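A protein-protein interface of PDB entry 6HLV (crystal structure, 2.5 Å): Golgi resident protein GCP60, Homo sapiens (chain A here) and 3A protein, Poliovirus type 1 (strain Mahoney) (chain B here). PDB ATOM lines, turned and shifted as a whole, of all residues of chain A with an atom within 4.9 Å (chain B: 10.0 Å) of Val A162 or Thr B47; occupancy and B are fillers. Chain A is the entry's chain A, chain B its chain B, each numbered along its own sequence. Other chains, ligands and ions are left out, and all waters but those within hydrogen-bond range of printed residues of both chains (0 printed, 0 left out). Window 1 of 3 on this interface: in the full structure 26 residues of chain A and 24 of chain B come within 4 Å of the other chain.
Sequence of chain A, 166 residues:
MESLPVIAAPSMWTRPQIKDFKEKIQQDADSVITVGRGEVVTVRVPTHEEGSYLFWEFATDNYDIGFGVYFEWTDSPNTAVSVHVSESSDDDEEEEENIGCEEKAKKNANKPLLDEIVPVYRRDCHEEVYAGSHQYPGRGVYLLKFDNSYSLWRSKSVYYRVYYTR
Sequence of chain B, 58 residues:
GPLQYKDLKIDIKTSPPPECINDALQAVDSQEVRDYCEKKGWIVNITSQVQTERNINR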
ATOM      1  N   SER A  31      22.317  36.633  12.849  1.00  0.00           N
ATOM      2  CA  SER A  31      23.076  35.416  12.588  1.00  0.00           C
ATOM      3  C   SER A  31      24.573  35.680  12.707  1.00  0.00           C
ATOM      4  O   SER A  31      25.386  34.778  12.508  1.00  0.00           O
ATOM      5  CB  SER A  31      22.749  34.862  11.199  1.00  0.00           C
ATOM      6  OG  SER A  31      21.418  34.382  11.137  1.00  0.00           O
ATOM      7  N   VAL A  45      19.459  26.000  20.881  1.00  0.00           N
ATOM      8  CA  VAL A  45      18.530  25.648  19.818  1.00  0.00           C
ATOM      9  C   VAL A  45      17.240  25.100  20.424  1.00  0.00           C
ATOM     10  O   VAL A  45      17.295  24.241  21.302  1.00  0.00           O
ATOM     11  CB  VAL A  45      19.138  24.601  18.870  1.00  0.00           C
ATOM     12  CG1 VAL A  45      18.222  24.357  17.678  1.00  0.00           C
ATOM     13  CG2 VAL A  45      20.512  25.049  18.406  1.00  0.00           C
ATOM     14  N   LEU A  54      19.993  17.745  13.924  1.00  0.00           N
ATOM     15  CA  LEU A  54      20.380  19.146  13.959  1.00  0.00           C
ATOM     16  C   LEU A  54      21.544  19.340  13.009  1.00  0.00           C
ATOM     17  O   LEU A  54      22.473  18.537  12.996  1.00  0.00           O
ATOM     18  CB  LEU A  54      20.773  19.588  15.369  1.00  0.00           C
ATOM     19  CG  LEU A  54      21.192  21.059  15.481  1.00  0.00           C
ATOM     20  CD1 LEU A  54      19.976  21.966  15.428  1.00  0.00           C
ATOM     21  CD2 LEU A  54      21.997  21.315  16.742  1.00  0.00           C
ATOM     22  N   PHE A  55      21.479  20.396  12.207  1.00  0.00           N
ATOM     23  CA  PHE A  55      22.593  20.791  11.357  1.00  0.00           C
ATOM     24  C   PHE A  55      23.069  22.161  11.796  1.00  0.00           C
ATOM     25  O   PHE A  55      22.259  23.040  12.078  1.00  0.00           O
ATOM     26  CB  PHE A  55      22.187  20.810   9.884  1.00  0.00           C
ATOM     27  CG  PHE A  55      21.793  19.467   9.351  1.00  0.00           C
ATOM     28  CD1 PHE A  55      20.472  19.064   9.366  1.00  0.00           C
ATOM     29  CD2 PHE A  55      22.747  18.605   8.840  1.00  0.00           C
ATOM     30  CE1 PHE A  55      20.107  17.829   8.879  1.00  0.00           C
ATOM     31  CE2 PHE A  55      22.388  17.366   8.353  1.00  0.00           C
ATOM     32  CZ  PHE A  55      21.066  16.977   8.372  1.00  0.00           C
ATOM     33  N   TRP A  56      24.385  22.325  11.872  1.00  0.00           N
ATOM     34  CA  TRP A  56      24.982  23.606  12.216  1.00  0.00           C
ATOM     35  C   TRP A  56      26.065  23.961  11.216  1.00  0.00           C
ATOM     36  O   TRP A  56      26.714  23.085  10.649  1.00  0.00           O
ATOM     37  CB  TRP A  56      25.568  23.577  13.634  1.00  0.00           C
ATOM     38  CG  TRP A  56      26.718  22.625  13.799  1.00  0.00           C
ATOM     39  CD1 TRP A  56      28.014  22.829  13.422  1.00  0.00           C
ATOM     40  CD2 TRP A  56      26.674  21.321  14.389  1.00  0.00           C
ATOM     41  NE1 TRP A  56      28.776  21.731  13.735  1.00  0.00           N
ATOM     42  CE2 TRP A  56      27.977  20.791  14.330  1.00  0.00           C
ATOM     43  CE3 TRP A  56      25.658  20.548  14.958  1.00  0.00           C
ATOM     44  CZ2 TRP A  56      28.291  19.527  14.820  1.00  0.00           C
ATOM     45  CZ3 TRP A  56      25.972  19.293  15.444  1.00  0.00           C
ATOM     46  CH2 TRP A  56      27.276  18.796  15.372  1.00  0.00           C
ATOM     47  N   LEU A 144      25.137  25.118  21.417  1.00  0.00           N
ATOM     48  CA  LEU A 144      26.318  25.368  20.605  1.00  0.00           C
ATOM     49  C   LEU A 144      27.213  26.347  21.344  1.00  0.00           C
ATOM     50  O   LEU A 144      26.834  27.493  21.579  1.00  0.00           O
ATOM     51  CB  LEU A 144      25.935  25.914  19.229  1.00  0.00           C
ATOM     52  CG  LEU A 144      24.844  25.142  18.485  1.00  0.00           C
ATOM     53  CD1 LEU A 144      24.513  25.818  17.165  1.00  0.00           C
ATOM     54  CD2 LEU A 144      25.262  23.701  18.256  1.00  0.00           C
ATOM     55  N   TYR A 160      26.936  32.231  11.942  1.00  0.00           N
ATOM     56  CA  TYR A 160      26.392  30.890  12.162  1.00  0.00           C
ATOM     57  C   TYR A 160      24.995  30.696  11.583  1.00  0.00           C
ATOM     58  O   TYR A 160      24.273  31.655  11.319  1.00  0.00           O
ATOM     59  CB  TYR A 160      26.368  30.568  13.660  1.00  0.00           C
ATOM     60  CG  TYR A 160      25.292  31.291  14.432  1.00  0.00           C
ATOM     61  CD1 TYR A 160      25.412  32.639  14.730  1.00  0.00           C
ATOM     62  CD2 TYR A 160      24.159  30.623  14.871  1.00  0.00           C
ATOM     63  CE1 TYR A 160      24.432  33.303  15.436  1.00  0.00           C
ATOM     64  CE2 TYR A 160      23.173  31.277  15.579  1.00  0.00           C
ATOM     65  CZ  TYR A 160      23.316  32.619  15.859  1.00  0.00           C
ATOM     66  OH  TYR A 160      22.339  33.281  16.562  1.00  0.00           O
ATOM     67  N   ARG A 161      24.636  29.431  11.379  1.00  0.00           N
ATOM     68  CA  ARG A 161      23.320  29.055  10.881  1.00  0.00           C
ATOM     69  C   ARG A 161      22.965  27.648  11.364  1.00  0.00           C
ATOM     70  O   ARG A 161      23.850  26.805  11.512  1.00  0.00           O
ATOM     71  CB  ARG A 161      23.295  29.119   9.352  1.00  0.00           C
ATOM     72  CG  ARG A 161      21.931  28.896   8.731  1.00  0.00           C
ATOM     73  CD  ARG A 161      22.058  28.384   7.309  1.00  0.00           C
ATOM     74  NE  ARG A 161      22.645  29.359   6.395  1.00  0.00           N
ATOM     75  CZ  ARG A 161      23.206  29.052   5.230  1.00  0.00           C
ATOM     76  NH1 ARG A 161      23.281  27.791   4.829  1.00  0.00           N
ATOM     77  NH2 ARG A 161      23.707  30.009   4.463  1.00  0.00           N
ATOM     78  N   VAL A 162      21.679  27.396  11.602  1.00  0.00           N
ATOM     79  CA  VAL A 162      21.226  26.068  12.012  1.00  0.00           C
ATOM     80  C   VAL A 162      19.922  25.637  11.335  1.00  0.00           C
ATOM     81  O   VAL A 162      19.009  26.441  11.145  1.00  0.00           O
ATOM     82  CB  VAL A 162      21.018  25.986  13.542  1.00  0.00           C
ATOM     83  CG1 VAL A 162      22.352  25.951  14.258  1.00  0.00           C
ATOM     84  CG2 VAL A 162      20.175  27.146  14.039  1.00  0.00           C
ATOM     85  N   TYR A 163      19.859  24.357  10.977  1.00  0.00           N
ATOM     86  CA  TYR A 163      18.635  23.723  10.496  1.00  0.00           C
ATOM     87  C   TYR A 163      18.290  22.515  11.355  1.00  0.00           C
ATOM     88  O   TYR A 163      19.134  22.021  12.102  1.00  0.00           O
ATOM     89  CB  TYR A 163      18.770  23.238   9.051  1.00  0.00           C
ATOM     90  CG  TYR A 163      19.129  24.263   8.007  1.00  0.00           C
ATOM     91  CD1 TYR A 163      18.144  24.898   7.264  1.00  0.00           C
ATOM     92  CD2 TYR A 163      20.454  24.555   7.723  1.00  0.00           C
ATOM     93  CE1 TYR A 163      18.468  25.816   6.288  1.00  0.00           C
ATOM     94  CE2 TYR A 163      20.787  25.470   6.747  1.00  0.00           C
ATOM     95  CZ  TYR A 163      19.790  26.097   6.032  1.00  0.00           C
ATOM     96  OH  TYR A 163      20.123  27.009   5.061  1.00  0.00           O
ATOM     97  N   TYR A 164      17.057  22.033  11.243  1.00  0.00           N
ATOM     98  CA  TYR A 164      16.755  20.665  11.654  1.00  0.00           C
ATOM     99  C   TYR A 164      15.859  20.000  10.618  1.00  0.00           C
ATOM    100  O   TYR A 164      15.258  20.673   9.783  1.00  0.00           O
ATOM    101  CB  TYR A 164      16.108  20.609  13.052  1.00  0.00           C
ATOM    102  CG  TYR A 164      14.709  21.196  13.197  1.00  0.00           C
ATOM    103  CD1 TYR A 164      13.639  20.730  12.439  1.00  0.00           C
ATOM    104  CD2 TYR A 164      14.453  22.179  14.141  1.00  0.00           C
ATOM    105  CE1 TYR A 164      12.372  21.256  12.587  1.00  0.00           C
ATOM    106  CE2 TYR A 164      13.184  22.708  14.298  1.00  0.00           C
ATOM    107  CZ  TYR A 164      12.149  22.242  13.520  1.00  0.00           C
ATOM    108  OH  TYR A 164      10.885  22.763  13.672  1.00  0.00           O
ATOM    109  N   LEU B  25      24.192  15.623   2.739  1.00  0.00           N
ATOM    110  CA  LEU B  25      24.794  16.907   3.079  1.00  0.00           C
ATOM    111  C   LEU B  25      26.284  16.816   3.380  1.00  0.00           C
ATOM    112  O   LEU B  25      26.976  17.818   3.329  1.00  0.00           O
ATOM    113  CB  LEU B  25      24.082  17.533   4.279  1.00  0.00           C
ATOM    114  CG  LEU B  25      22.912  18.467   3.972  1.00  0.00           C
ATOM    115  CD1 LEU B  25      22.241  18.910   5.259  1.00  0.00           C
ATOM    116  CD2 LEU B  25      23.377  19.677   3.180  1.00  0.00           C
ATOM    117  N   ARG B  34      20.982  22.861   0.205  1.00  0.00           N
ATOM    118  CA  ARG B  34      20.266  23.243   1.414  1.00  0.00           C
ATOM    119  C   ARG B  34      18.987  23.986   1.054  1.00  0.00           C
ATOM    120  O   ARG B  34      17.955  23.810   1.701  1.00  0.00           O
ATOM    121  CB  ARG B  34      21.158  24.096   2.319  1.00  0.00           C
ATOM    122  CG  ARG B  34      22.239  23.287   3.029  1.00  0.00           C
ATOM    123  CD  ARG B  34      23.213  24.158   3.807  1.00  0.00           C
ATOM    124  NE  ARG B  34      24.295  23.364   4.390  1.00  0.00           N
ATOM    125  CZ  ARG B  34      24.274  22.829   5.607  1.00  0.00           C
ATOM    126  NH1 ARG B  34      23.226  22.992   6.404  1.00  0.00           N
ATOM    127  NH2 ARG B  34      25.312  22.124   6.035  1.00  0.00           N
ATOM    128  N   GLU B  38      15.153  22.703   1.805  1.00  0.00           N
ATOM    129  CA  GLU B  38      14.284  23.619   2.537  1.00  0.00           C
ATOM    130  C   GLU B  38      13.004  23.900   1.752  1.00  0.00           C
ATOM    131  O   GLU B  38      11.942  24.093   2.341  1.00  0.00           O
ATOM    132  CB  GLU B  38      15.010  24.930   2.847  1.00  0.00           C
ATOM    133  CG  GLU B  38      14.278  25.803   3.859  1.00  0.00           C
ATOM    134  CD  GLU B  38      15.015  27.088   4.185  1.00  0.00           C
ATOM    135  OE1 GLU B  38      16.156  27.267   3.708  1.00  0.00           O
ATOM    136  OE2 GLU B  38      14.452  27.922   4.923  1.00  0.00           O
ATOM    137  N   ILE B  43      14.044  20.244   5.521  1.00  0.00           N
ATOM    138  CA  ILE B  43      14.763  20.941   6.583  1.00  0.00           C
ATOM    139  C   ILE B  43      14.165  22.325   6.819  1.00  0.00           C
ATOM    140  O   ILE B  43      13.537  22.901   5.932  1.00  0.00           O
ATOM    141  CB  ILE B  43      16.272  21.079   6.264  1.00  0.00           C
ATOM    142  CG1 ILE B  43      16.502  21.968   5.039  1.00  0.00           C
ATOM    143  CG2 ILE B  43      16.890  19.706   6.042  1.00  0.00           C
ATOM    144  CD1 ILE B  43      17.961  22.284   4.790  1.00  0.00           C
ATOM    145  N   VAL B  44      14.369  22.846   8.025  1.00  0.00           N
ATOM    146  CA  VAL B  44      13.819  24.134   8.429  1.00  0.00           C
ATOM    147  C   VAL B  44      14.904  24.999   9.053  1.00  0.00           C
ATOM    148  O   VAL B  44      15.677  24.518   9.875  1.00  0.00           O
ATOM    149  CB  VAL B  44      12.673  23.959   9.442  1.00  0.00           C
ATOM    150  CG1 VAL B  44      12.078  25.304   9.812  1.00  0.00           C
ATOM    151  CG2 VAL B  44      11.607  23.029   8.883  1.00  0.00           C
ATOM    152  N   ASN B  45      14.946  26.277   8.686  1.00  0.00           N
ATOM    153  CA  ASN B  45      15.967  27.176   9.209  1.00  0.00           C
ATOM    154  C   ASN B  45      15.456  27.878  10.463  1.00  0.00           C
ATOM    155  O   ASN B  45      14.609  28.767  10.394  1.00  0.00           O
ATOM    156  CB  ASN B  45      16.360  28.196   8.139  1.00  0.00           C
ATOM    157  CG  ASN B  45      17.553  29.042   8.537  1.00  0.00           C
ATOM    158  OD1 ASN B  45      17.723  29.403   9.700  1.00  0.00           O
ATOM    159  ND2 ASN B  45      18.388  29.368   7.559  1.00  0.00           N
ATOM    160  N   ILE B  46      15.999  27.460  11.602  1.00  0.00           N
ATOM    161  CA  ILE B  46      15.570  27.928  12.923  1.00  0.00           C
ATOM    162  C   ILE B  46      16.478  28.987  13.543  1.00  0.00           C
ATOM    163  O   ILE B  46      16.272  29.379  14.690  1.00  0.00           O
ATOM    164  CB  ILE B  46      15.463  26.752  13.910  1.00  0.00           C
ATOM    165  CG1 ILE B  46      16.820  26.055  14.055  1.00  0.00           C
ATOM    166  CG2 ILE B  46      14.388  25.783  13.449  1.00  0.00           C
ATOM    167  CD1 ILE B  46      16.767  24.758  14.806  1.00  0.00           C
ATOM    168  N   THR B  47      17.490  29.422  12.802  1.00  0.00           N
ATOM    169  CA  THR B  47      18.533  30.292  13.345  1.00  0.00           C
ATOM    170  C   THR B  47      17.989  31.508  14.096  1.00  0.00           C
ATOM    171  O   THR B  47      18.588  31.960  15.072  1.00  0.00           O
ATOM    172  CB  THR B  47      19.463  30.789  12.231  1.00  0.00           C
ATOM    173  OG1 THR B  47      19.941  29.673  11.472  1.00  0.00           O
ATOM    174  CG2 THR B  47      20.646  31.544  12.816  1.00  0.00           C
ATOM    175  N   SER B  48      16.852  32.029  13.648  1.00  0.00           N
ATOM    176  CA  SER B  48      16.268  33.222  14.254  1.00  0.00           C
ATOM    177  C   SER B  48      15.575  32.926  15.584  1.00  0.00           C
ATOM    178  O   SER B  48      15.309  33.839  16.364  1.00  0.00           O
ATOM    179  CB  SER B  48      15.271  33.863  13.288  1.00  0.00           C
ATOM    180  OG  SER B  48      14.230  32.961  12.956  1.00  0.00           O
ATOM    181  N   GLN B  49      15.287  31.653  15.837  1.00  0.00           N
ATOM    182  CA  GLN B  49      14.502  31.248  17.004  1.00  0.00           C
ATOM    183  C   GLN B  49      15.343  30.818  18.210  1.00  0.00           C
ATOM    184  O   GLN B  49      14.804  30.343  19.207  1.00  0.00           O
ATOM    185  CB  GLN B  49      13.554  30.119  16.606  1.00  0.00           C
ATOM    186  CG  GLN B  49      12.362  30.605  15.800  1.00  0.00           C
ATOM    187  CD  GLN B  49      11.800  29.540  14.886  1.00  0.00           C
ATOM    188  OE1 GLN B  49      11.214  28.559  15.341  1.00  0.00           O
ATOM    189  NE2 GLN B  49      11.980  29.728  13.584  1.00  0.00           N
ATOM    190  N   VAL B  50      16.659  30.961  18.111  1.00  0.00           N
ATOM    191  CA  VAL B  50      17.558  30.557  19.189  1.00  0.00           C
ATOM    192  C   VAL B  50      17.579  31.539  20.365  1.00  0.00           C
ATOM    193  O   VAL B  50      17.214  32.705  20.222  1.00  0.00           O
ATOM    194  CB  VAL B  50      19.000  30.395  18.673  1.00  0.00           C
ATOM    195  CG1 VAL B  50      19.053  29.379  17.543  1.00  0.00           C
ATOM    196  CG2 VAL B  50      19.554  31.731  18.214  1.00  0.00           C
ATOM    197  N   GLN B  51      18.004  31.042  21.526  1.00  0.00           N
ATOM    198  CA  GLN B  51      18.343  31.879  22.679  1.00  0.00           C
ATOM    199  C   GLN B  51      19.857  32.003  22.781  1.00  0.00           C
ATOM    200  O   GLN B  51      20.576  31.069  22.430  1.00  0.00           O
ATOM    201  CB  GLN B  51      17.800  31.291  23.982  1.00  0.00           C
ATOM    202  CG  GLN B  51      16.318  31.469  24.218  1.00  0.00           C
ATOM    203  CD  GLN B  51      15.892  30.910  25.564  1.00  0.00           C
ATOM    204  OE1 GLN B  51      16.730  30.596  26.410  1.00  0.00           O
ATOM    205  NE2 GLN B  51      14.587  30.784  25.770  1.00  0.00           N
ATOM    206  N   THR B  52      20.342  33.149  23.254  1.00  0.00           N
ATOM    207  CA  THR B  52      21.775  33.328  23.490  1.00  0.00           C
ATOM    208  C   THR B  52      22.077  33.648  24.952  1.00  0.00           C
ATOM    209  O   THR B  52      21.376  34.432  25.593  1.00  0.00           O
ATOM    210  CB  THR B  52      22.365  34.441  22.611  1.00  0.00           C
ATOM    211  OG1 THR B  52      21.818  35.707  22.995  1.00  0.00           O
ATOM    212  CG2 THR B  52      22.070  34.172  21.144  1.00  0.00           C
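Along chain B the printed residues that touch a printed residue of chain A span positions 25 to 50.
Among the printed residues, 19 pairs touch across the chains.
O of Val A162 sits at hydrogen-bond distance from N of Ile B46 (3.2 Å).
The backbone NH (N) of Val B44 lies within hydrogen-bond range of the backbone carbonyl oxygen (O) of Tyr A164 (2.9 Å).
The backbone NH of Val A162 is in hydrogen-bond range of the side-chain hydroxyl of Thr B47, 2.9 Å away.
The side-chain hydroxyl of Thr B47 is in hydrogen-bond range of the side-chain amide oxygen of Asn B45.
NH1 of Arg A161 sits at hydrogen-bond distance from OH of Tyr A163, at 3.3 Å.
The backbone carbonyl oxygen (O) of Tyr A163 lies within hydrogen-bond range of the backbone NH (N) of Phe A55 (2.9 Å).
The backbone carbonyl oxygen of Ser A31 sits at hydrogen-bond distance from the backbone NH of Tyr A160.
Of the printed residues of chain B, Val A162 touches Asn B45, Ile B46 and Thr B47.
Of the printed residues of chain B, Tyr A164 touches Ile B43 (3.2 Å), Val B44 (2.9 Å) and Ile B46 (3.4 Å).
Of the printed residues of chain A, Ile B46 touches Val A45 (3.2 Å), Val A162 (3.2 Å) and Tyr A164 (3.4 Å).
Thr B47 touches four residues of chain A.
Gln B51 touches none of the printed residues of chain A.
The nearest printed residue of chain A that does not touch Thr B47 is Tyr A163 (5.3 Å).
Among the printed residues, merely in contact across the chains: Ser A31 with Thr B47 (3.4 Å), Val A45 with Ile B46 (3.2 Å), Phe A55 with Leu B25 (3.5 Å), Tyr A160 with Thr B47 (3.8 Å), Tyr A160 with Val B50 (3.6 Å), Arg A161 with Arg B34 (3.8 Å), Arg A161 with Asn B45 (3.8 Å), Arg A161 with Thr B47 (3.5 Å), Val A162 with Asn B45 (3.5 Å), Tyr A163 with Arg B34 (3.4 Å), Tyr A163 with Glu B38 (3.8 Å), Tyr A163 with Ile B43 (3.6 Å), Tyr A163 with Val B44 (3.1 Å), Tyr A163 with Asn B45 (3.7 Å), Tyr A164 with Ile B43 (3.2 Å) and Tyr A164 with Ile B46 (3.4 Å).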
